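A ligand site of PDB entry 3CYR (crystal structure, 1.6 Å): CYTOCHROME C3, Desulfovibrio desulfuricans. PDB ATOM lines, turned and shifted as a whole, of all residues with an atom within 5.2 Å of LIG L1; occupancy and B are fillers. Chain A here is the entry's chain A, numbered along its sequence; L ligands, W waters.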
ATOM      1  N   ALA A   1     -23.511   6.436  -5.942  1.00  0.00           N
ATOM      2  CA  ALA A   1     -23.080   7.000  -7.237  1.00  0.00           C
ATOM      3  C   ALA A   1     -23.913   6.378  -8.346  1.00  0.00           C
ATOM      4  O   ALA A   1     -24.505   5.310  -8.146  1.00  0.00           O
ATOM      5  CB  ALA A   1     -21.595   6.643  -7.447  1.00  0.00           C
ATOM      6  N   PRO A   2     -23.961   7.018  -9.506  1.00  0.00           N
ATOM      7  CA  PRO A   2     -24.700   6.314 -10.606  1.00  0.00           C
ATOM      8  C   PRO A   2     -23.820   5.183 -11.106  1.00  0.00           C
ATOM      9  O   PRO A   2     -22.606   5.139 -10.771  1.00  0.00           O
ATOM     10  CB  PRO A   2     -24.919   7.378 -11.657  1.00  0.00           C
ATOM     11  CG  PRO A   2     -24.609   8.676 -10.983  1.00  0.00           C
ATOM     12  CD  PRO A   2     -23.472   8.337 -10.019  1.00  0.00           C
ATOM     13  N   ALA A   3     -24.367   4.263 -11.872  1.00  0.00           N
ATOM     14  CA  ALA A   3     -23.538   3.197 -12.416  1.00  0.00           C
ATOM     15  C   ALA A   3     -22.563   3.777 -13.463  1.00  0.00           C
ATOM     16  O   ALA A   3     -22.894   4.671 -14.233  1.00  0.00           O
ATOM     17  CB  ALA A   3     -24.527   2.256 -13.213  1.00  0.00           C
ATOM     18  N   VAL A   4     -21.370   3.221 -13.494  1.00  0.00           N
ATOM     19  CA  VAL A   4     -20.448   3.732 -14.560  1.00  0.00           C
ATOM     20  C   VAL A   4     -20.881   3.168 -15.899  1.00  0.00           C
ATOM     21  O   VAL A   4     -21.412   2.050 -16.006  1.00  0.00           O
ATOM     22  CB  VAL A   4     -19.010   3.441 -14.195  1.00  0.00           C
ATOM     23  CG1 VAL A   4     -18.756   2.066 -13.672  1.00  0.00           C
ATOM     24  CG2 VAL A   4     -18.016   3.881 -15.228  1.00  0.00           C
ATOM     25  N   PRO A   5     -20.759   3.986 -16.966  1.00  0.00           N
ATOM     26  CA  PRO A   5     -21.125   3.512 -18.306  1.00  0.00           C
ATOM     27  C   PRO A   5     -20.261   2.329 -18.721  1.00  0.00           C
ATOM     28  O   PRO A   5     -19.062   2.307 -18.480  1.00  0.00           O
ATOM     29  CB  PRO A   5     -20.851   4.716 -19.204  1.00  0.00           C
ATOM     30  CG  PRO A   5     -20.998   5.883 -18.290  1.00  0.00           C
ATOM     31  CD  PRO A   5     -20.322   5.401 -16.990  1.00  0.00           C
ATOM     32  N   VAL A   9     -17.914   6.324 -24.363  1.00  0.00           N
ATOM     33  CA  VAL A   9     -18.788   7.508 -24.523  1.00  0.00           C
ATOM     34  C   VAL A   9     -18.086   8.619 -25.269  1.00  0.00           C
ATOM     35  O   VAL A   9     -16.860   8.711 -25.238  1.00  0.00           O
ATOM     36  CB  VAL A   9     -19.293   8.003 -23.166  1.00  0.00           C
ATOM     37  CG1 VAL A   9     -20.182   6.953 -22.501  1.00  0.00           C
ATOM     38  CG2 VAL A   9     -18.186   8.427 -22.217  1.00  0.00           C
ATOM     39  N   GLU A  10     -18.878   9.494 -25.936  1.00  0.00           N
ATOM     40  CA  GLU A  10     -18.258  10.583 -26.684  1.00  0.00           C
ATOM     41  C   GLU A  10     -17.781  11.724 -25.754  1.00  0.00           C
ATOM     42  O   GLU A  10     -18.579  12.180 -24.916  1.00  0.00           O
ATOM     43  CB  GLU A  10     -19.332  11.286 -27.573  1.00  0.00           C
ATOM     44  CG  GLU A  10     -20.353  10.393 -28.195  1.00  0.00           C
ATOM     45  CD  GLU A  10     -21.604  11.187 -28.654  1.00  0.00           C
ATOM     46  OE1 GLU A  10     -22.465  11.517 -27.787  1.00  0.00           O
ATOM     47  OE2 GLU A  10     -21.639  11.485 -29.843  1.00  0.00           O
ATOM     48  N   VAL A  11     -16.646  12.271 -26.091  1.00  0.00           N
ATOM     49  CA  VAL A  11     -16.115  13.528 -25.490  1.00  0.00           C
ATOM     50  C   VAL A  11     -15.975  14.483 -26.701  1.00  0.00           C
ATOM     51  O   VAL A  11     -15.079  14.294 -27.539  1.00  0.00           O
ATOM     52  CB  VAL A  11     -14.763  13.329 -24.836  1.00  0.00           C
ATOM     53  CG1 VAL A  11     -14.314  14.601 -24.085  1.00  0.00           C
ATOM     54  CG2 VAL A  11     -14.931  12.218 -23.718  1.00  0.00           C
ATOM     55  N   PHE A  20     -14.242   7.791 -24.986  1.00  0.00           N
ATOM     56  CA  PHE A  20     -13.543   7.491 -23.695  1.00  0.00           C
ATOM     57  C   PHE A  20     -14.074   6.190 -23.103  1.00  0.00           C
ATOM     58  O   PHE A  20     -15.284   6.072 -22.828  1.00  0.00           O
ATOM     59  CB  PHE A  20     -13.936   8.648 -22.694  1.00  0.00           C
ATOM     60  CG  PHE A  20     -13.410   8.297 -21.277  1.00  0.00           C
ATOM     61  CD1 PHE A  20     -12.052   8.432 -21.012  1.00  0.00           C
ATOM     62  CD2 PHE A  20     -14.256   7.839 -20.296  1.00  0.00           C
ATOM     63  CE1 PHE A  20     -11.542   8.067 -19.773  1.00  0.00           C
ATOM     64  CE2 PHE A  20     -13.760   7.453 -19.036  1.00  0.00           C
ATOM     65  CZ  PHE A  20     -12.390   7.586 -18.792  1.00  0.00           C
ATOM     66  N   HIS A  22     -14.378   3.579 -19.901  1.00  0.00           N
ATOM     67  CA  HIS A  22     -14.165   3.503 -18.438  1.00  0.00           C
ATOM     68  C   HIS A  22     -13.423   2.240 -18.025  1.00  0.00           C
ATOM     69  O   HIS A  22     -12.742   2.226 -16.980  1.00  0.00           O
ATOM     70  CB  HIS A  22     -15.539   3.547 -17.720  1.00  0.00           C
ATOM     71  CG  HIS A  22     -16.072   4.950 -17.478  1.00  0.00           C
ATOM     72  ND1 HIS A  22     -16.796   5.635 -18.418  1.00  0.00           N
ATOM     73  CD2 HIS A  22     -15.959   5.766 -16.410  1.00  0.00           C
ATOM     74  CE1 HIS A  22     -17.112   6.833 -17.935  1.00  0.00           C
ATOM     75  NE2 HIS A  22     -16.585   6.978 -16.738  1.00  0.00           N
ATOM     76  N   HIS A  25      -9.923   2.033 -16.824  1.00  0.00           N
ATOM     77  CA  HIS A  25      -9.659   2.947 -15.705  1.00  0.00           C
ATOM     78  C   HIS A  25     -10.384   2.482 -14.435  1.00  0.00           C
ATOM     79  O   HIS A  25     -10.602   3.291 -13.539  1.00  0.00           O
ATOM     80  CB  HIS A  25     -10.205   4.350 -16.084  1.00  0.00           C
ATOM     81  CG  HIS A  25      -9.502   4.956 -17.277  1.00  0.00           C
ATOM     82  ND1 HIS A  25     -10.064   4.929 -18.535  1.00  0.00           N
ATOM     83  CD2 HIS A  25      -8.310   5.564 -17.418  1.00  0.00           C
ATOM     84  CE1 HIS A  25      -9.276   5.531 -19.400  1.00  0.00           C
ATOM     85  NE2 HIS A  25      -8.189   5.923 -18.753  1.00  0.00           N
ATOM     86  N   VAL A  28      -8.934   3.394 -11.120  1.00  0.00           N
ATOM     87  CA  VAL A  28      -8.713   4.821 -10.760  1.00  0.00           C
ATOM     88  C   VAL A  28      -9.972   5.297 -10.014  1.00  0.00           C
ATOM     89  O   VAL A  28     -11.110   5.022 -10.468  1.00  0.00           O
ATOM     90  CB  VAL A  28      -8.575   5.659 -12.073  1.00  0.00           C
ATOM     91  CG1 VAL A  28      -8.502   7.162 -11.779  1.00  0.00           C
ATOM     92  CG2 VAL A  28      -7.328   5.233 -12.853  1.00  0.00           C
ATOM     93  N   GLU A  29      -9.799   6.029  -8.908  1.00  0.00           N
ATOM     94  CA  GLU A  29     -10.938   6.560  -8.137  1.00  0.00           C
ATOM     95  C   GLU A  29     -11.798   7.478  -9.009  1.00  0.00           C
ATOM     96  O   GLU A  29     -11.286   8.264  -9.777  1.00  0.00           O
ATOM     97  CB  GLU A  29     -10.425   7.409  -6.950  1.00  0.00           C
ATOM     98  CG  GLU A  29      -9.784   6.511  -5.870  1.00  0.00           C
ATOM     99  CD  GLU A  29      -9.108   7.313  -4.789  1.00  0.00           C
ATOM    100  OE1 GLU A  29      -9.227   8.549  -4.749  1.00  0.00           O
ATOM    101  OE2 GLU A  29      -8.406   6.696  -3.945  1.00  0.00           O
ATOM    102  N   CYS A  30     -13.131   7.377  -8.861  1.00  0.00           N
ATOM    103  CA  CYS A  30     -13.993   8.237  -9.682  1.00  0.00           C
ATOM    104  C   CYS A  30     -13.609   9.715  -9.517  1.00  0.00           C
ATOM    105  O   CYS A  30     -13.629  10.476 -10.467  1.00  0.00           O
ATOM    106  CB  CYS A  30     -15.487   8.061  -9.429  1.00  0.00           C
ATOM    107  SG  CYS A  30     -16.155   6.444  -9.149  1.00  0.00           S
ATOM    108  N   CYS A  33     -11.170  12.062 -11.691  1.00  0.00           N
ATOM    109  CA  CYS A  33     -11.633  12.737 -12.905  1.00  0.00           C
ATOM    110  C   CYS A  33     -12.890  13.568 -12.594  1.00  0.00           C
ATOM    111  O   CYS A  33     -12.936  14.734 -12.958  1.00  0.00           O
ATOM    112  CB  CYS A  33     -11.974  11.658 -13.984  1.00  0.00           C
ATOM    113  SG  CYS A  33     -10.479  10.632 -14.349  1.00  0.00           S
ATOM    114  N   HIS A  34     -13.877  12.950 -11.973  1.00  0.00           N
ATOM    115  CA  HIS A  34     -15.156  13.671 -11.618  1.00  0.00           C
ATOM    116  C   HIS A  34     -14.878  14.376 -10.271  1.00  0.00           C
ATOM    117  O   HIS A  34     -15.307  13.895  -9.240  1.00  0.00           O
ATOM    118  CB  HIS A  34     -16.247  12.613 -11.465  1.00  0.00           C
ATOM    119  CG  HIS A  34     -16.557  11.858 -12.753  1.00  0.00           C
ATOM    120  ND1 HIS A  34     -17.113  12.482 -13.839  1.00  0.00           N
ATOM    121  CD2 HIS A  34     -16.312  10.594 -13.122  1.00  0.00           C
ATOM    122  CE1 HIS A  34     -17.239  11.591 -14.845  1.00  0.00           C
ATOM    123  NE2 HIS A  34     -16.786  10.422 -14.424  1.00  0.00           N
ATOM    124  N   TYR A  43     -21.199  14.401 -11.427  1.00  0.00           N
ATOM    125  CA  TYR A  43     -20.822  13.544 -12.544  1.00  0.00           C
ATOM    126  C   TYR A  43     -21.305  14.158 -13.859  1.00  0.00           C
ATOM    127  O   TYR A  43     -21.492  13.459 -14.850  1.00  0.00           O
ATOM    128  CB  TYR A  43     -21.484  12.163 -12.339  1.00  0.00           C
ATOM    129  CG  TYR A  43     -20.922  11.455 -11.124  1.00  0.00           C
ATOM    130  CD1 TYR A  43     -19.817  10.648 -11.213  1.00  0.00           C
ATOM    131  CD2 TYR A  43     -21.525  11.601  -9.874  1.00  0.00           C
ATOM    132  CE1 TYR A  43     -19.284   9.999 -10.120  1.00  0.00           C
ATOM    133  CE2 TYR A  43     -20.992  10.978  -8.768  1.00  0.00           C
ATOM    134  CZ  TYR A  43     -19.882  10.176  -8.889  1.00  0.00           C
ATOM    135  OH  TYR A  43     -19.369   9.519  -7.803  1.00  0.00           O
ATOM    136  N   ALA A  44     -21.495  15.479 -13.857  1.00  0.00           N
ATOM    137  CA  ALA A  44     -21.875  16.171 -15.083  1.00  0.00           C
ATOM    138  C   ALA A  44     -20.785  16.138 -16.148  1.00  0.00           C
ATOM    139  O   ALA A  44     -19.580  16.040 -15.910  1.00  0.00           O
ATOM    140  CB  ALA A  44     -22.264  17.614 -14.763  1.00  0.00           C
ATOM    141  N   LYS A  45     -21.211  16.318 -17.417  1.00  0.00           N
ATOM    142  CA  LYS A  45     -20.216  16.350 -18.502  1.00  0.00           C
ATOM    143  C   LYS A  45     -19.192  17.415 -18.325  1.00  0.00           C
ATOM    144  O   LYS A  45     -19.510  18.545 -17.864  1.00  0.00           O
ATOM    145  CB  LYS A  45     -20.949  16.455 -19.849  1.00  0.00           C
ATOM    146  CG  LYS A  45     -21.774  15.161 -20.102  1.00  0.00           C
ATOM    147  CD  LYS A  45     -22.293  15.220 -21.558  1.00  0.00           C
ATOM    148  CE  LYS A  45     -23.259  14.039 -21.769  1.00  0.00           C
ATOM    149  NZ  LYS A  45     -24.307  14.373 -22.789  1.00  0.00           N
ATOM    150  N   CYS A  46     -17.914  17.120 -18.619  1.00  0.00           N
ATOM    151  CA  CYS A  46     -16.854  18.089 -18.382  1.00  0.00           C
ATOM    152  C   CYS A  46     -17.089  19.426 -19.055  1.00  0.00           C
ATOM    153  O   CYS A  46     -16.701  20.458 -18.475  1.00  0.00           O
ATOM    154  CB  CYS A  46     -15.472  17.518 -18.748  1.00  0.00           C
ATOM    155  SG  CYS A  46     -15.185  15.804 -18.327  1.00  0.00           S
ATOM    156  N   GLY A  47     -17.650  19.413 -20.250  1.00  0.00           N
ATOM    157  CA  GLY A  47     -17.876  20.600 -21.050  1.00  0.00           C
ATOM    158  C   GLY A  47     -19.239  21.245 -20.859  1.00  0.00           C
ATOM    159  O   GLY A  47     -19.640  22.049 -21.742  1.00  0.00           O
HETATM  160  C1  LIG L   1     -18.636   9.995 -18.056  1.00  0.00           C
HETATM  161  C2  LIG L   1     -19.518   7.814 -13.799  1.00  0.00           C
HETATM  162  C3  LIG L   1     -14.775   7.066 -13.188  1.00  0.00           C
HETATM  163  C4  LIG L   1     -13.926  10.087 -16.907  1.00  0.00           C
HETATM  164  C5  LIG L   1     -19.288   9.449 -16.982  1.00  0.00           C
HETATM  165  C6  LIG L   1     -20.735   9.395 -16.796  1.00  0.00           C
HETATM  166  C7  LIG L   1     -20.968   8.858 -15.601  1.00  0.00           C
HETATM  167  C8  LIG L   1     -19.699   8.445 -15.032  1.00  0.00           C
HETATM  168  C9  LIG L   1     -22.324   8.713 -14.881  1.00  0.00           C
HETATM  169  C10 LIG L   1     -21.758   9.991 -17.808  1.00  0.00           C
HETATM  170  C11 LIG L   1     -21.925  11.513 -17.738  1.00  0.00           C
HETATM  171  C12 LIG L   1     -23.165  12.090 -18.369  1.00  0.00           C
HETATM  172  O1  LIG L   1     -23.848  12.909 -17.683  1.00  0.00           O
HETATM  173  O2  LIG L   1     -23.424  11.740 -19.552  1.00  0.00           O
HETATM  174  C13 LIG L   1     -18.307   7.427 -13.239  1.00  0.00           C
HETATM  175  C14 LIG L   1     -18.122   6.716 -12.000  1.00  0.00           C
HETATM  176  C15 LIG L   1     -16.821   6.477 -11.791  1.00  0.00           C
HETATM  177  C16 LIG L   1     -16.142   7.034 -12.978  1.00  0.00           C
HETATM  178  C17 LIG L   1     -19.354   6.335 -11.115  1.00  0.00           C
HETATM  179  C18 LIG L   1     -16.091   5.613 -10.757  1.00  0.00           C
HETATM  180  C19 LIG L   1     -16.535   4.261 -10.726  1.00  0.00           C
HETATM  181  C20 LIG L   1     -14.152   7.826 -14.174  1.00  0.00           C
HETATM  182  C21 LIG L   1     -12.727   8.030 -14.280  1.00  0.00           C
HETATM  183  C22 LIG L   1     -12.438   8.946 -15.202  1.00  0.00           C
HETATM  184  C23 LIG L   1     -13.712   9.256 -15.856  1.00  0.00           C
HETATM  185  C24 LIG L   1     -11.703   7.298 -13.334  1.00  0.00           C
HETATM  186  C25 LIG L   1     -11.095   9.511 -15.641  1.00  0.00           C
HETATM  187  C26 LIG L   1     -10.115   8.504 -16.007  1.00  0.00           C
HETATM  188  C27 LIG L   1     -15.107  10.319 -17.605  1.00  0.00           C
HETATM  189  C28 LIG L   1     -15.284  11.115 -18.790  1.00  0.00           C
HETATM  190  C29 LIG L   1     -16.618  11.082 -19.104  1.00  0.00           C
HETATM  191  C30 LIG L   1     -17.273  10.279 -18.121  1.00  0.00           C
HETATM  192  C31 LIG L   1     -14.217  11.915 -19.534  1.00  0.00           C
HETATM  193  C32 LIG L   1     -17.271  11.810 -20.314  1.00  0.00           C
HETATM  194  C33 LIG L   1     -17.765  13.251 -19.968  1.00  0.00           C
HETATM  195  C34 LIG L   1     -18.141  14.110 -21.146  1.00  0.00           C
HETATM  196  O3  LIG L   1     -18.598  13.576 -22.159  1.00  0.00           O
HETATM  197  O4  LIG L   1     -17.894  15.354 -21.050  1.00  0.00           O
HETATM  198  N1  LIG L   1     -18.703   8.814 -15.896  1.00  0.00           N
HETATM  199  N2  LIG L   1     -17.064   7.630 -13.849  1.00  0.00           N
HETATM  200  N3  LIG L   1     -14.752   8.547 -15.187  1.00  0.00           N
HETATM  201  N4  LIG L   1     -16.355   9.819 -17.163  1.00  0.00           N
HETATM  202 FE1  LIG L   1     -16.728   8.703 -15.531  1.00  0.00          FE
HETATM  203  C1  LG2 L   2      -5.839   3.655 -20.924  1.00  0.00           C
HETATM  204  C2  LG2 L   2      -8.144   7.651 -22.450  1.00  0.00           C
HETATM  205  C3  LG2 L   2      -7.334   9.696 -18.110  1.00  0.00           C
HETATM  206  C4  LG2 L   2      -4.761   5.839 -16.706  1.00  0.00           C
HETATM  207  C5  LG2 L   2      -6.507   4.566 -21.733  1.00  0.00           C
HETATM  208  C6  LG2 L   2      -6.924   4.350 -23.102  1.00  0.00           C
HETATM  209  C7  LG2 L   2      -7.588   5.421 -23.506  1.00  0.00           C
HETATM  210  C8  LG2 L   2      -7.569   6.386 -22.426  1.00  0.00           C
HETATM  211  C9  LG2 L   2      -8.181   5.718 -24.904  1.00  0.00           C
HETATM  212  C10 LG2 L   2      -6.507   3.063 -23.904  1.00  0.00           C
HETATM  213  C11 LG2 L   2      -7.495   1.887 -23.667  1.00  0.00           C
HETATM  214  C12 LG2 L   2      -7.744   1.025 -24.871  1.00  0.00           C
HETATM  215  O1  LG2 L   2      -6.836   0.961 -25.736  1.00  0.00           O
HETATM  216  O2  LG2 L   2      -8.870   0.443 -24.898  1.00  0.00           O
HETATM  217  C13 LG2 L   2      -8.125   8.558 -21.388  1.00  0.00           C
HETATM  218  C14 LG2 L   2      -8.640   9.913 -21.436  1.00  0.00           C
HETATM  219  C15 LG2 L   2      -8.446  10.518 -20.254  1.00  0.00           C
HETATM  220  C16 LG2 L   2      -7.745   9.511 -19.430  1.00  0.00           C
HETATM  221  C17 LG2 L   2      -9.314  10.485 -22.715  1.00  0.00           C
HETATM  222  C18 LG2 L   2      -8.932  11.857 -19.720  1.00  0.00           C
HETATM  223  C19 LG2 L   2     -10.368  12.021 -19.730  1.00  0.00           C
HETATM  224  C20 LG2 L   2      -6.563   8.809 -17.373  1.00  0.00           C
HETATM  225  C21 LG2 L   2      -6.071   9.083 -16.008  1.00  0.00           C
HETATM  226  C22 LG2 L   2      -5.288   8.071 -15.633  1.00  0.00           C
HETATM  227  C23 LG2 L   2      -5.340   7.099 -16.700  1.00  0.00           C
HETATM  228  C24 LG2 L   2      -6.350  10.418 -15.305  1.00  0.00           C
HETATM  229  C25 LG2 L   2      -4.427   7.900 -14.353  1.00  0.00           C
HETATM  230  C26 LG2 L   2      -4.907   8.512 -13.193  1.00  0.00           C
HETATM  231  C27 LG2 L   2      -4.883   4.876 -17.702  1.00  0.00           C
HETATM  232  C28 LG2 L   2      -4.378   3.531 -17.650  1.00  0.00           C
HETATM  233  C29 LG2 L   2      -4.702   2.903 -18.787  1.00  0.00           C
HETATM  234  C30 LG2 L   2      -5.390   3.878 -19.636  1.00  0.00           C
HETATM  235  C31 LG2 L   2      -3.585   2.928 -16.445  1.00  0.00           C
HETATM  236  C32 LG2 L   2      -4.330   1.469 -19.195  1.00  0.00           C
HETATM  237  C33 LG2 L   2      -2.828   1.290 -19.519  1.00  0.00           C
HETATM  238  C34 LG2 L   2      -2.343  -0.144 -19.513  1.00  0.00           C
HETATM  239  O3  LG2 L   2      -2.883  -0.908 -20.327  1.00  0.00           O
HETATM  240  O4  LG2 L   2      -1.413  -0.404 -18.692  1.00  0.00           O
HETATM  241  N1  LG2 L   2      -6.888   5.830 -21.341  1.00  0.00           N
HETATM  242  N2  LG2 L   2      -7.546   8.346 -20.142  1.00  0.00           N
HETATM  243  N3  LG2 L   2      -6.096   7.597 -17.781  1.00  0.00           N
HETATM  244  N4  LG2 L   2      -5.482   5.071 -18.959  1.00  0.00           N
HETATM  245 FE1  LG2 L   2      -6.467   6.703 -19.562  1.00  0.00          FE
HETATM  246  C1  LG3 L   3     -10.623  22.430 -12.643  1.00  0.00           C
HETATM  247  C2  LG3 L   3     -10.828  18.360 -15.299  1.00  0.00           C
HETATM  248  C3  LG3 L   3     -15.601  18.272 -14.645  1.00  0.00           C
HETATM  249  C4  LG3 L   3     -15.434  22.844 -13.069  1.00  0.00           C
HETATM  250  C5  LG3 L   3     -10.262  21.291 -13.338  1.00  0.00           C
HETATM  251  C6  LG3 L   3      -8.895  20.901 -13.663  1.00  0.00           C
HETATM  252  C7  LG3 L   3      -8.936  19.778 -14.374  1.00  0.00           C
HETATM  253  C8  LG3 L   3     -10.361  19.420 -14.546  1.00  0.00           C
HETATM  254  C9  LG3 L   3      -7.802  18.966 -14.955  1.00  0.00           C
HETATM  255  C10 LG3 L   3      -7.654  21.765 -13.254  1.00  0.00           C
HETATM  256  C11 LG3 L   3      -7.365  22.909 -14.212  1.00  0.00           C
HETATM  257  C12 LG3 L   3      -6.320  23.907 -13.783  1.00  0.00           C
HETATM  258  O1  LG3 L   3      -5.527  23.612 -12.867  1.00  0.00           O
HETATM  259  O2  LG3 L   3      -6.306  24.977 -14.476  1.00  0.00           O
HETATM  260  C13 LG3 L   3     -12.172  18.011 -15.464  1.00  0.00           C
HETATM  261  C14 LG3 L   3     -12.694  16.927 -16.261  1.00  0.00           C
HETATM  262  C15 LG3 L   3     -14.036  16.875 -16.101  1.00  0.00           C
HETATM  263  C16 LG3 L   3     -14.368  17.979 -15.194  1.00  0.00           C
HETATM  264  C17 LG3 L   3     -11.805  15.986 -17.105  1.00  0.00           C
HETATM  265  C18 LG3 L   3     -15.047  15.785 -16.524  1.00  0.00           C
HETATM  266  C19 LG3 L   3     -14.718  14.486 -15.996  1.00  0.00           C
HETATM  267  C20 LG3 L   3     -16.006  19.542 -14.221  1.00  0.00           C
HETATM  268  C21 LG3 L   3     -17.388  19.995 -14.048  1.00  0.00           C
HETATM  269  C22 LG3 L   3     -17.347  21.308 -13.752  1.00  0.00           C
HETATM  270  C23 LG3 L   3     -15.948  21.650 -13.547  1.00  0.00           C
HETATM  271  C24 LG3 L   3     -18.593  19.054 -14.252  1.00  0.00           C
HETATM  272  C25 LG3 L   3     -18.518  22.281 -13.480  1.00  0.00           C
HETATM  273  C26 LG3 L   3     -19.309  21.878 -12.361  1.00  0.00           C
HETATM  274  C27 LG3 L   3     -14.115  23.075 -12.707  1.00  0.00           C
HETATM  275  C28 LG3 L   3     -13.644  24.260 -12.005  1.00  0.00           C
HETATM  276  C29 LG3 L   3     -12.326  24.141 -11.858  1.00  0.00           C
HETATM  277  C30 LG3 L   3     -11.916  22.878 -12.458  1.00  0.00           C
HETATM  278  C31 LG3 L   3     -14.567  25.411 -11.548  1.00  0.00           C
HETATM  279  C32 LG3 L   3     -11.335  25.175 -11.252  1.00  0.00           C
HETATM  280  C33 LG3 L   3     -11.170  25.103  -9.728  1.00  0.00           C
HETATM  281  C34 LG3 L   3     -10.814  23.731  -9.209  1.00  0.00           C
HETATM  282  O3  LG3 L   3     -11.690  23.105  -8.595  1.00  0.00           O
HETATM  283  O4  LG3 L   3      -9.640  23.326  -9.462  1.00  0.00           O
HETATM  284  N1  LG3 L   3     -11.125  20.388 -13.937  1.00  0.00           N
HETATM  285  N2  LG3 L   3     -13.232  18.750 -14.939  1.00  0.00           N
HETATM  286  N3  LG3 L   3     -15.140  20.560 -13.881  1.00  0.00           N
HETATM  287  N4  LG3 L   3     -13.048  22.230 -12.900  1.00  0.00           N
HETATM  288 FE1  LG3 L   3     -13.114  20.511 -13.916  1.00  0.00          FE
HETATM  289  O   HOH W   1     -21.011  11.146 -20.707  1.00  0.00           O
HETATM  290  O   HOH W   2     -13.265   3.855 -11.845  1.00  0.00           O
HETATM  291  O   HOH W   3     -19.184  13.422 -16.878  1.00  0.00           O
HETATM  292  O   HOH W   4     -21.012  11.825 -23.685  1.00  0.00           O
HETATM  293  O   HOH W   5     -18.245  17.658 -22.184  1.00  0.00           O
HETATM  294  O   HOH W   6     -19.003  15.248 -24.555  1.00  0.00           O
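The side-chain sulfur of Cys 30 is covalently linked to a carbon (C18) of LIG L1 (1.8 Å).
C25 of LIG L1 is covalently linked to SG of Cys 33 (1.8 Å).
An iron atom (FE1) of LIG L1 is bound by a ring nitrogen (NE2) of His 34, at 2.0 Å.
FE1 of LIG L1 is bound by NE2 of His 22, at 2.1 Å.
The backbone NH (N) of Cys 46 sits at hydrogen-bond distance from an oxygen (O4) of LIG L1, 3.0 Å away.
An oxygen (O3) of LIG L1 lies close to the backbone carbonyl oxygen (O) of Glu 10 (3.1 Å).
A ring nitrogen (NE2) of His 25 is bound to an iron atom (FE1) of LG2 L2 (2.1 Å).
A carbon (C18) of LG3 L3 is bonded to the side-chain sulfur (SG) of Cys 46.
The backbone NH (N) of Phe 20 is in hydrogen-bond range of the backbone carbonyl oxygen (O) of Val 9 (2.8 Å).
Residues that only touch LIG L1: Pro 2 (3.5 Å), Pro 5 (3.7 Å), Val 9 (3.99 Å), Phe 20 (3.4 Å), His 25 (3.7 Å), Val 28 (3.6 Å), Glu 29 (3.7 Å), Tyr 43 (3.5 Å) and Lys 45 (3.2 Å).
Hydrophobic or aromatic side chains within 4 Å of LIG L1: Pro 5, Val 9, Phe 20, His 22, His 25, Val 28, His 34 and Tyr 43.
Of the 21 residues printed, 15 come within 4 Å of LIG L1.
Water W5 bridges an oxygen (O4) of LIG L1 (2.6 Å) and the backbone NH (N) of Gly 47 (2.7 Å).
Water W6 bridges an oxygen (O3) of LIG L1 (2.9 Å) and the backbone carbonyl oxygen (O) of Glu 10 (3.1 Å).
Water W4 lies within hydrogen-bond range of the backbone carbonyl oxygen of Glu 10 and an oxygen (O3) of LIG L1.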
